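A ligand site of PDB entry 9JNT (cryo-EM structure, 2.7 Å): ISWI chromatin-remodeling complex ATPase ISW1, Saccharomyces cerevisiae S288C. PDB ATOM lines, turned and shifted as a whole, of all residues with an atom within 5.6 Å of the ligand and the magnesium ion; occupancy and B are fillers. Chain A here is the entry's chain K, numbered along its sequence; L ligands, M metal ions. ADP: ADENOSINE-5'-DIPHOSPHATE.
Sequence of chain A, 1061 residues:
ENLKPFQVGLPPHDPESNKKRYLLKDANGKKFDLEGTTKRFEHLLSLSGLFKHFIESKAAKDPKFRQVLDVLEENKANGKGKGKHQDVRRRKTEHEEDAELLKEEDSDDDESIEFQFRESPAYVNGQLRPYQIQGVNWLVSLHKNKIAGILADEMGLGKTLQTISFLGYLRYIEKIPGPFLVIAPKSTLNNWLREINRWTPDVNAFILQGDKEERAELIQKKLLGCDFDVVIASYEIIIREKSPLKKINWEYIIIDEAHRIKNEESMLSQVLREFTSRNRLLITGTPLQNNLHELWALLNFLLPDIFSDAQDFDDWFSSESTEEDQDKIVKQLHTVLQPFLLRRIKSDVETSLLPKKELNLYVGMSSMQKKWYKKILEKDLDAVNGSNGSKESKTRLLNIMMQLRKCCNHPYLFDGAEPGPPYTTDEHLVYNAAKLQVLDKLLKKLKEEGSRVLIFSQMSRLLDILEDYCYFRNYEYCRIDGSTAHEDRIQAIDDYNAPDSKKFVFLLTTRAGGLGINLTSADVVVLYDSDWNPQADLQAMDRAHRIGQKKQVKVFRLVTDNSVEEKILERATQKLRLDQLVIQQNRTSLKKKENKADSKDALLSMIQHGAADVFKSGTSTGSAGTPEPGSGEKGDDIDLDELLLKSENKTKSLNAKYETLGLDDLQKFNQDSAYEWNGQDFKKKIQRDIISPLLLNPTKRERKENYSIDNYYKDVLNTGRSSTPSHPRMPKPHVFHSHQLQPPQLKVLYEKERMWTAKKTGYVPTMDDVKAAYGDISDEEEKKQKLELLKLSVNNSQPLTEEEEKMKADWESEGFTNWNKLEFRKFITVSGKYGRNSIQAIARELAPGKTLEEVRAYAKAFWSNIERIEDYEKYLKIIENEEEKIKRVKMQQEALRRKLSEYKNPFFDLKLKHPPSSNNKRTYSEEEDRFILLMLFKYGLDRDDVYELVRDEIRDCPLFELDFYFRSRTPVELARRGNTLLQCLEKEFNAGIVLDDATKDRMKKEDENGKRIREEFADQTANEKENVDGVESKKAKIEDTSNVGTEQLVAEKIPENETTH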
ATOM      1  N   GLY A 126     -30.611  -4.068  -3.398  1.00  0.00           N
ATOM      2  CA  GLY A 126     -29.230  -3.678  -3.631  1.00  0.00           C
ATOM      3  C   GLY A 126     -28.214  -4.724  -3.237  1.00  0.00           C
ATOM      4  O   GLY A 126     -28.560  -5.845  -2.875  1.00  0.00           O
ATOM      5  N   GLN A 127     -26.933  -4.363  -3.311  1.00  0.00           N
ATOM      6  CA  GLN A 127     -25.854  -5.248  -2.928  1.00  0.00           C
ATOM      7  C   GLN A 127     -25.363  -4.895  -1.532  1.00  0.00           C
ATOM      8  O   GLN A 127     -25.499  -3.761  -1.072  1.00  0.00           O
ATOM      9  CB  GLN A 127     -24.693  -5.163  -3.933  1.00  0.00           C
ATOM     10  CG  GLN A 127     -23.722  -6.336  -3.863  1.00  0.00           C
ATOM     11  CD  GLN A 127     -24.308  -7.635  -4.380  1.00  0.00           C
ATOM     12  OE1 GLN A 127     -25.451  -7.679  -4.835  1.00  0.00           O
ATOM     13  NE2 GLN A 127     -23.525  -8.701  -4.327  1.00  0.00           N
ATOM     14  N   LEU A 128     -24.784  -5.890  -0.856  1.00  0.00           N
ATOM     15  CA  LEU A 128     -24.358  -5.769   0.527  1.00  0.00           C
ATOM     16  C   LEU A 128     -22.875  -6.076   0.612  1.00  0.00           C
ATOM     17  O   LEU A 128     -22.412  -7.076   0.054  1.00  0.00           O
ATOM     18  CB  LEU A 128     -25.186  -6.698   1.414  1.00  0.00           C
ATOM     19  CG  LEU A 128     -25.182  -6.567   2.932  1.00  0.00           C
ATOM     20  CD1 LEU A 128     -26.522  -7.021   3.479  1.00  0.00           C
ATOM     21  CD2 LEU A 128     -24.088  -7.413   3.513  1.00  0.00           C
ATOM     22  N   ARG A 129     -22.125  -5.215   1.304  1.00  0.00           N
ATOM     23  CA  ARG A 129     -20.668  -5.303   1.287  1.00  0.00           C
ATOM     24  C   ARG A 129     -20.182  -6.581   1.982  1.00  0.00           C
ATOM     25  O   ARG A 129     -20.806  -7.059   2.929  1.00  0.00           O
ATOM     26  CB  ARG A 129     -20.055  -4.076   1.962  1.00  0.00           C
ATOM     27  CG  ARG A 129     -20.256  -2.793   1.165  1.00  0.00           C
ATOM     28  CD  ARG A 129     -20.024  -1.557   2.016  1.00  0.00           C
ATOM     29  NE  ARG A 129     -20.612  -0.362   1.417  1.00  0.00           N
ATOM     30  CZ  ARG A 129     -20.872   0.755   2.084  1.00  0.00           C
ATOM     31  NH1 ARG A 129     -20.595   0.844   3.375  1.00  0.00           N
ATOM     32  NH2 ARG A 129     -21.416   1.789   1.455  1.00  0.00           N
ATOM     33  N   GLN A 132     -19.846  -6.509   5.662  1.00  0.00           N
ATOM     34  CA  GLN A 132     -21.186  -6.550   6.243  1.00  0.00           C
ATOM     35  C   GLN A 132     -21.777  -7.947   6.143  1.00  0.00           C
ATOM     36  O   GLN A 132     -22.550  -8.352   7.020  1.00  0.00           O
ATOM     37  CB  GLN A 132     -22.089  -5.522   5.558  1.00  0.00           C
ATOM     38  CG  GLN A 132     -21.569  -4.103   5.616  1.00  0.00           C
ATOM     39  CD  GLN A 132     -22.252  -3.200   4.607  1.00  0.00           C
ATOM     40  OE1 GLN A 132     -22.810  -3.678   3.615  1.00  0.00           O
ATOM     41  NE2 GLN A 132     -22.204  -1.899   4.857  1.00  0.00           N
ATOM     42  N   GLU A 154     -17.193   1.108  13.723  1.00  0.00           N
ATOM     43  CA  GLU A 154     -17.054   2.546  13.897  1.00  0.00           C
ATOM     44  C   GLU A 154     -18.200   3.298  13.240  1.00  0.00           C
ATOM     45  O   GLU A 154     -18.886   2.786  12.349  1.00  0.00           O
ATOM     46  CB  GLU A 154     -15.720   3.033  13.334  1.00  0.00           C
ATOM     47  CG  GLU A 154     -14.523   2.676  14.188  1.00  0.00           C
ATOM     48  CD  GLU A 154     -13.885   1.381  13.751  1.00  0.00           C
ATOM     49  OE1 GLU A 154     -14.443   0.738  12.835  1.00  0.00           O
ATOM     50  OE2 GLU A 154     -12.848   1.000  14.317  1.00  0.00           O
ATOM     51  N   MET A 155     -18.402   4.526  13.696  1.00  0.00           N
ATOM     52  CA  MET A 155     -19.448   5.377  13.154  1.00  0.00           C
ATOM     53  C   MET A 155     -19.252   5.591  11.659  1.00  0.00           C
ATOM     54  O   MET A 155     -18.127   5.854  11.199  1.00  0.00           O
ATOM     55  CB  MET A 155     -19.452   6.725  13.888  1.00  0.00           C
ATOM     56  CG  MET A 155     -20.540   7.706  13.480  1.00  0.00           C
ATOM     57  SD  MET A 155     -20.149   8.653  11.993  1.00  0.00           S
ATOM     58  CE  MET A 155     -18.890   9.751  12.637  1.00  0.00           C
ATOM     59  N   GLY A 156     -20.338   5.462  10.896  1.00  0.00           N
ATOM     60  CA  GLY A 156     -20.303   5.621   9.467  1.00  0.00           C
ATOM     61  C   GLY A 156     -19.920   4.380   8.689  1.00  0.00           C
ATOM     62  O   GLY A 156     -19.979   4.401   7.453  1.00  0.00           O
ATOM     63  N   LEU A 157     -19.536   3.302   9.376  1.00  0.00           N
ATOM     64  CA  LEU A 157     -19.199   2.078   8.673  1.00  0.00           C
ATOM     65  C   LEU A 157     -20.425   1.353   8.143  1.00  0.00           C
ATOM     66  O   LEU A 157     -20.315   0.571   7.200  1.00  0.00           O
ATOM     67  CB  LEU A 157     -18.408   1.145   9.599  1.00  0.00           C
ATOM     68  CG  LEU A 157     -17.613   0.036   8.914  1.00  0.00           C
ATOM     69  CD1 LEU A 157     -16.883   0.579   7.703  1.00  0.00           C
ATOM     70  CD2 LEU A 157     -16.647  -0.594   9.886  1.00  0.00           C
ATOM     71  N   GLY A 158     -21.591   1.602   8.728  1.00  0.00           N
ATOM     72  CA  GLY A 158     -22.818   0.934   8.311  1.00  0.00           C
ATOM     73  C   GLY A 158     -23.198  -0.175   9.257  1.00  0.00           C
ATOM     74  O   GLY A 158     -22.662  -1.282   9.177  1.00  0.00           O
ATOM     75  N   LYS A 159     -24.133   0.094  10.170  1.00  0.00           N
ATOM     76  CA  LYS A 159     -24.546  -0.900  11.146  1.00  0.00           C
ATOM     77  C   LYS A 159     -26.048  -1.103  11.098  1.00  0.00           C
ATOM     78  O   LYS A 159     -26.540  -2.205  11.342  1.00  0.00           O
ATOM     79  CB  LYS A 159     -24.107  -0.482  12.551  1.00  0.00           C
ATOM     80  CG  LYS A 159     -22.642  -0.117  12.657  1.00  0.00           C
ATOM     81  CD  LYS A 159     -22.237   0.161  14.093  1.00  0.00           C
ATOM     82  CE  LYS A 159     -22.475   1.620  14.449  1.00  0.00           C
ATOM     83  NZ  LYS A 159     -21.954   1.938  15.803  1.00  0.00           N
ATOM     84  N   THR A 160     -26.793  -0.035  10.781  1.00  0.00           N
ATOM     85  CA  THR A 160     -28.241  -0.173  10.649  1.00  0.00           C
ATOM     86  C   THR A 160     -28.600  -1.119   9.513  1.00  0.00           C
ATOM     87  O   THR A 160     -29.526  -1.932   9.643  1.00  0.00           O
ATOM     88  CB  THR A 160     -28.870   1.202  10.407  1.00  0.00           C
ATOM     89  OG1 THR A 160     -28.404   1.731   9.169  1.00  0.00           O
ATOM     90  CG2 THR A 160     -28.509   2.159  11.535  1.00  0.00           C
ATOM     91  N   LEU A 161     -27.867  -1.040   8.403  1.00  0.00           N
ATOM     92  CA  LEU A 161     -28.113  -1.964   7.303  1.00  0.00           C
ATOM     93  C   LEU A 161     -27.894  -3.401   7.740  1.00  0.00           C
ATOM     94  O   LEU A 161     -28.691  -4.289   7.433  1.00  0.00           O
ATOM     95  CB  LEU A 161     -27.204  -1.610   6.118  1.00  0.00           C
ATOM     96  CG  LEU A 161     -27.428  -2.301   4.764  1.00  0.00           C
ATOM     97  CD1 LEU A 161     -26.926  -1.399   3.653  1.00  0.00           C
ATOM     98  CD2 LEU A 161     -26.722  -3.638   4.699  1.00  0.00           C
ATOM     99  N   THR A 188     -32.248  10.016  15.212  1.00  0.00           N
ATOM    100  CA  THR A 188     -31.933   8.931  14.288  1.00  0.00           C
ATOM    101  C   THR A 188     -33.166   8.189  13.782  1.00  0.00           C
ATOM    102  O   THR A 188     -33.068   7.468  12.788  1.00  0.00           O
ATOM    103  CB  THR A 188     -30.979   7.958  14.986  1.00  0.00           C
ATOM    104  OG1 THR A 188     -29.869   8.688  15.537  1.00  0.00           O
ATOM    105  CG2 THR A 188     -30.410   6.947  14.000  1.00  0.00           C
ATOM    106  N   ASN A 191     -33.958   8.255  10.164  1.00  0.00           N
ATOM    107  CA  ASN A 191     -32.860   7.584   9.478  1.00  0.00           C
ATOM    108  C   ASN A 191     -32.854   6.078   9.724  1.00  0.00           C
ATOM    109  O   ASN A 191     -32.088   5.368   9.071  1.00  0.00           O
ATOM    110  CB  ASN A 191     -31.524   8.185   9.893  1.00  0.00           C
ATOM    111  CG  ASN A 191     -30.468   8.051   8.825  1.00  0.00           C
ATOM    112  OD1 ASN A 191     -30.731   7.538   7.740  1.00  0.00           O
ATOM    113  ND2 ASN A 191     -29.256   8.516   9.119  1.00  0.00           N
ATOM    114  N   GLU A 195     -34.228   3.325   6.056  1.00  0.00           N
ATOM    115  CA  GLU A 195     -33.596   2.068   5.705  1.00  0.00           C
ATOM    116  C   GLU A 195     -34.547   0.888   5.850  1.00  0.00           C
ATOM    117  O   GLU A 195     -34.501  -0.054   5.050  1.00  0.00           O
ATOM    118  CB  GLU A 195     -32.337   1.860   6.556  1.00  0.00           C
ATOM    119  CG  GLU A 195     -31.118   2.644   6.076  1.00  0.00           C
ATOM    120  CD  GLU A 195     -31.166   4.117   6.434  1.00  0.00           C
ATOM    121  OE1 GLU A 195     -32.262   4.706   6.461  1.00  0.00           O
ATOM    122  OE2 GLU A 195     -30.091   4.698   6.683  1.00  0.00           O
ATOM    123  N   ARG A 198     -36.471   0.988   2.734  1.00  0.00           N
ATOM    124  CA  ARG A 198     -35.699   0.861   1.496  1.00  0.00           C
ATOM    125  C   ARG A 198     -35.145  -0.533   1.305  1.00  0.00           C
ATOM    126  O   ARG A 198     -35.356  -1.146   0.249  1.00  0.00           O
ATOM    127  CB  ARG A 198     -34.580   1.902   1.478  1.00  0.00           C
ATOM    128  CG  ARG A 198     -33.558   1.683   0.373  1.00  0.00           C
ATOM    129  CD  ARG A 198     -32.822   2.968   0.071  1.00  0.00           C
ATOM    130  NE  ARG A 198     -31.716   2.745  -0.858  1.00  0.00           N
ATOM    131  CZ  ARG A 198     -30.436   2.783  -0.496  1.00  0.00           C
ATOM    132  NH1 ARG A 198     -30.097   3.043   0.761  1.00  0.00           N
ATOM    133  NH2 ARG A 198     -29.484   2.562  -1.400  1.00  0.00           N
ATOM    134  N   TRP A 199     -34.434  -1.076   2.292  1.00  0.00           N
ATOM    135  CA  TRP A 199     -33.721  -2.332   2.075  1.00  0.00           C
ATOM    136  C   TRP A 199     -34.671  -3.525   2.059  1.00  0.00           C
ATOM    137  O   TRP A 199     -34.536  -4.410   1.219  1.00  0.00           O
ATOM    138  CB  TRP A 199     -32.643  -2.503   3.136  1.00  0.00           C
ATOM    139  CG  TRP A 199     -31.527  -1.520   2.992  1.00  0.00           C
ATOM    140  CD1 TRP A 199     -31.057  -0.662   3.945  1.00  0.00           C
ATOM    141  CD2 TRP A 199     -30.744  -1.285   1.816  1.00  0.00           C
ATOM    142  NE1 TRP A 199     -30.034   0.090   3.436  1.00  0.00           N
ATOM    143  CE2 TRP A 199     -29.821  -0.272   2.134  1.00  0.00           C
ATOM    144  CE3 TRP A 199     -30.728  -1.822   0.530  1.00  0.00           C
ATOM    145  CZ2 TRP A 199     -28.894   0.206   1.214  1.00  0.00           C
ATOM    146  CZ3 TRP A 199     -29.809  -1.350  -0.388  1.00  0.00           C
ATOM    147  CH2 TRP A 199     -28.910  -0.343  -0.034  1.00  0.00           C
ATOM    148  N   ASP A 256     -29.482   1.122  19.354  1.00  0.00           N
ATOM    149  CA  ASP A 256     -28.422   1.845  18.669  1.00  0.00           C
ATOM    150  C   ASP A 256     -27.822   2.880  19.608  1.00  0.00           C
ATOM    151  O   ASP A 256     -28.509   3.476  20.430  1.00  0.00           O
ATOM    152  CB  ASP A 256     -28.965   2.521  17.412  1.00  0.00           C
ATOM    153  CG  ASP A 256     -27.865   2.933  16.445  1.00  0.00           C
ATOM    154  OD1 ASP A 256     -26.821   3.451  16.903  1.00  0.00           O
ATOM    155  OD2 ASP A 256     -28.053   2.750  15.233  1.00  0.00           O
ATOM    156  N   GLU A 257     -26.511   3.084  19.470  1.00  0.00           N
ATOM    157  CA  GLU A 257     -25.753   4.011  20.325  1.00  0.00           C
ATOM    158  C   GLU A 257     -25.938   3.646  21.796  1.00  0.00           C
ATOM    159  O   GLU A 257     -26.504   4.405  22.585  1.00  0.00           O
ATOM    160  CB  GLU A 257     -26.162   5.464  20.059  1.00  0.00           C
ATOM    161  CG  GLU A 257     -25.830   5.964  18.651  1.00  0.00           C
ATOM    162  CD  GLU A 257     -24.454   5.538  18.186  1.00  0.00           C
ATOM    163  OE1 GLU A 257     -24.332   5.095  17.021  1.00  0.00           O
ATOM    164  OE2 GLU A 257     -23.483   5.665  18.964  1.00  0.00           O
ATOM    165  N   ILE A 283     -25.980  -1.967  19.696  1.00  0.00           N
ATOM    166  CA  ILE A 283     -25.170  -1.323  18.671  1.00  0.00           C
ATOM    167  C   ILE A 283     -24.556  -0.087  19.286  1.00  0.00           C
ATOM    168  O   ILE A 283     -25.271   0.772  19.814  1.00  0.00           O
ATOM    169  CB  ILE A 283     -26.007  -0.963  17.427  1.00  0.00           C
ATOM    170  CG1 ILE A 283     -26.706  -2.202  16.877  1.00  0.00           C
ATOM    171  CG2 ILE A 283     -25.112  -0.355  16.368  1.00  0.00           C
ATOM    172  CD1 ILE A 283     -25.754  -3.235  16.344  1.00  0.00           C
HETATM  173  PB  ADP L   1     -24.208   3.738  11.597  1.00  0.00           P
HETATM  174  O1B ADP L   1     -23.092   4.755  11.545  1.00  0.00           O
HETATM  175  O2B ADP L   1     -24.747   3.495  12.982  1.00  0.00           O
HETATM  176  O3B ADP L   1     -23.950   2.493  10.792  1.00  0.00           O
HETATM  177  PA  ADP L   1     -25.282   5.027   9.346  1.00  0.00           P
HETATM  178  O1A ADP L   1     -24.226   6.106   9.357  1.00  0.00           O
HETATM  179  O2A ADP L   1     -26.654   5.333   8.788  1.00  0.00           O
HETATM  180  O3A ADP L   1     -25.428   4.463  10.843  1.00  0.00           O
HETATM  181  O5' ADP L   1     -24.707   3.796   8.483  1.00  0.00           O
HETATM  182  C5' ADP L   1     -25.519   3.161   7.499  1.00  0.00           C
HETATM  183  C4' ADP L   1     -24.856   3.450   6.161  1.00  0.00           C
HETATM  184  O4' ADP L   1     -24.987   2.401   5.185  1.00  0.00           O
HETATM  185  C3' ADP L   1     -25.429   4.683   5.497  1.00  0.00           C
HETATM  186  O3' ADP L   1     -24.671   5.831   5.863  1.00  0.00           O
HETATM  187  C2' ADP L   1     -25.282   4.413   4.009  1.00  0.00           C
HETATM  188  O2' ADP L   1     -24.398   5.365   3.413  1.00  0.00           O
HETATM  189  C1' ADP L   1     -24.688   3.016   3.939  1.00  0.00           C
HETATM  190  N9  ADP L   1     -25.167   2.273   2.748  1.00  0.00           N
HETATM  191  C8  ADP L   1     -26.066   2.737   1.849  1.00  0.00           C
HETATM  192  N7  ADP L   1     -26.272   1.838   0.861  1.00  0.00           N
HETATM  193  C5  ADP L   1     -25.486   0.776   1.110  1.00  0.00           C
HETATM  194  C6  ADP L   1     -25.215  -0.526   0.458  1.00  0.00           C
HETATM  195  N6  ADP L   1     -25.843  -0.894  -0.683  1.00  0.00           N
HETATM  196  N1  ADP L   1     -24.316  -1.345   1.043  1.00  0.00           N
HETATM  197  C2  ADP L   1     -23.684  -1.000   2.178  1.00  0.00           C
HETATM  198  N3  ADP L   1     -23.876   0.156   2.826  1.00  0.00           N
HETATM  199  C4  ADP L   1     -24.746   1.075   2.344  1.00  0.00           C
HETATM  200 MG    MG M   1     -25.464   5.345  13.010  1.00  0.00          MG
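O3B of the ligand is in hydrogen-bond range of N of Lys 159. The backbone carbonyl oxygen (O) of Gln 127 lies within hydrogen-bond range of a nitrogen (N6) of the ligand (2.9 Å). An oxygen (O1B) of the ligand lies within hydrogen-bond range of the backbone NH (N) of Gly 156 (2.9 Å). The backbone NH of Gly 158 lies close to an oxygen (O3B) of the ligand, at 3.3 Å. N3 of the ligand lies close to NH2 of Arg 129 (3.3 Å). The side-chain amide nitrogen (NE2) of Gln 132 sits close to a nitrogen (N3) of the ligand (3.3 Å).
The backbone NH (N) of Arg 129 is in hydrogen-bond range of the side-chain amide oxygen (OE1) of Gln 132, 2.9 Å away.
Met 155 touches the ligand (C to O1B, 3.9 Å). Thr 160 touches the ligand. Leu 161 touches the ligand (CD1 to N3, 3.5 Å). NH2 of Arg 198 touches N7 of the ligand (3.99 Å). Trp 199 touches the ligand (CZ2 to N7, 3.1 Å). 11 residues have an atom within 4 Å of the ligand: Gln 127, Arg 129, Gln 132, Met 155, Gly 156, Gly 158, Lys 159, Thr 160, Leu 161, Arg 198 and Trp 199.
No residue comes within 4 Å of the magnesium ion. The nearest printed residue that does not touch the magnesium ion is Glu 257 (4.2 Å).
The magnesium ion is bound by O2B of the ligand (2.0 Å) and O3A of the ligand (2.3 Å). Slightly farther from the magnesium ion lies O1B of the ligand (2.8 Å).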
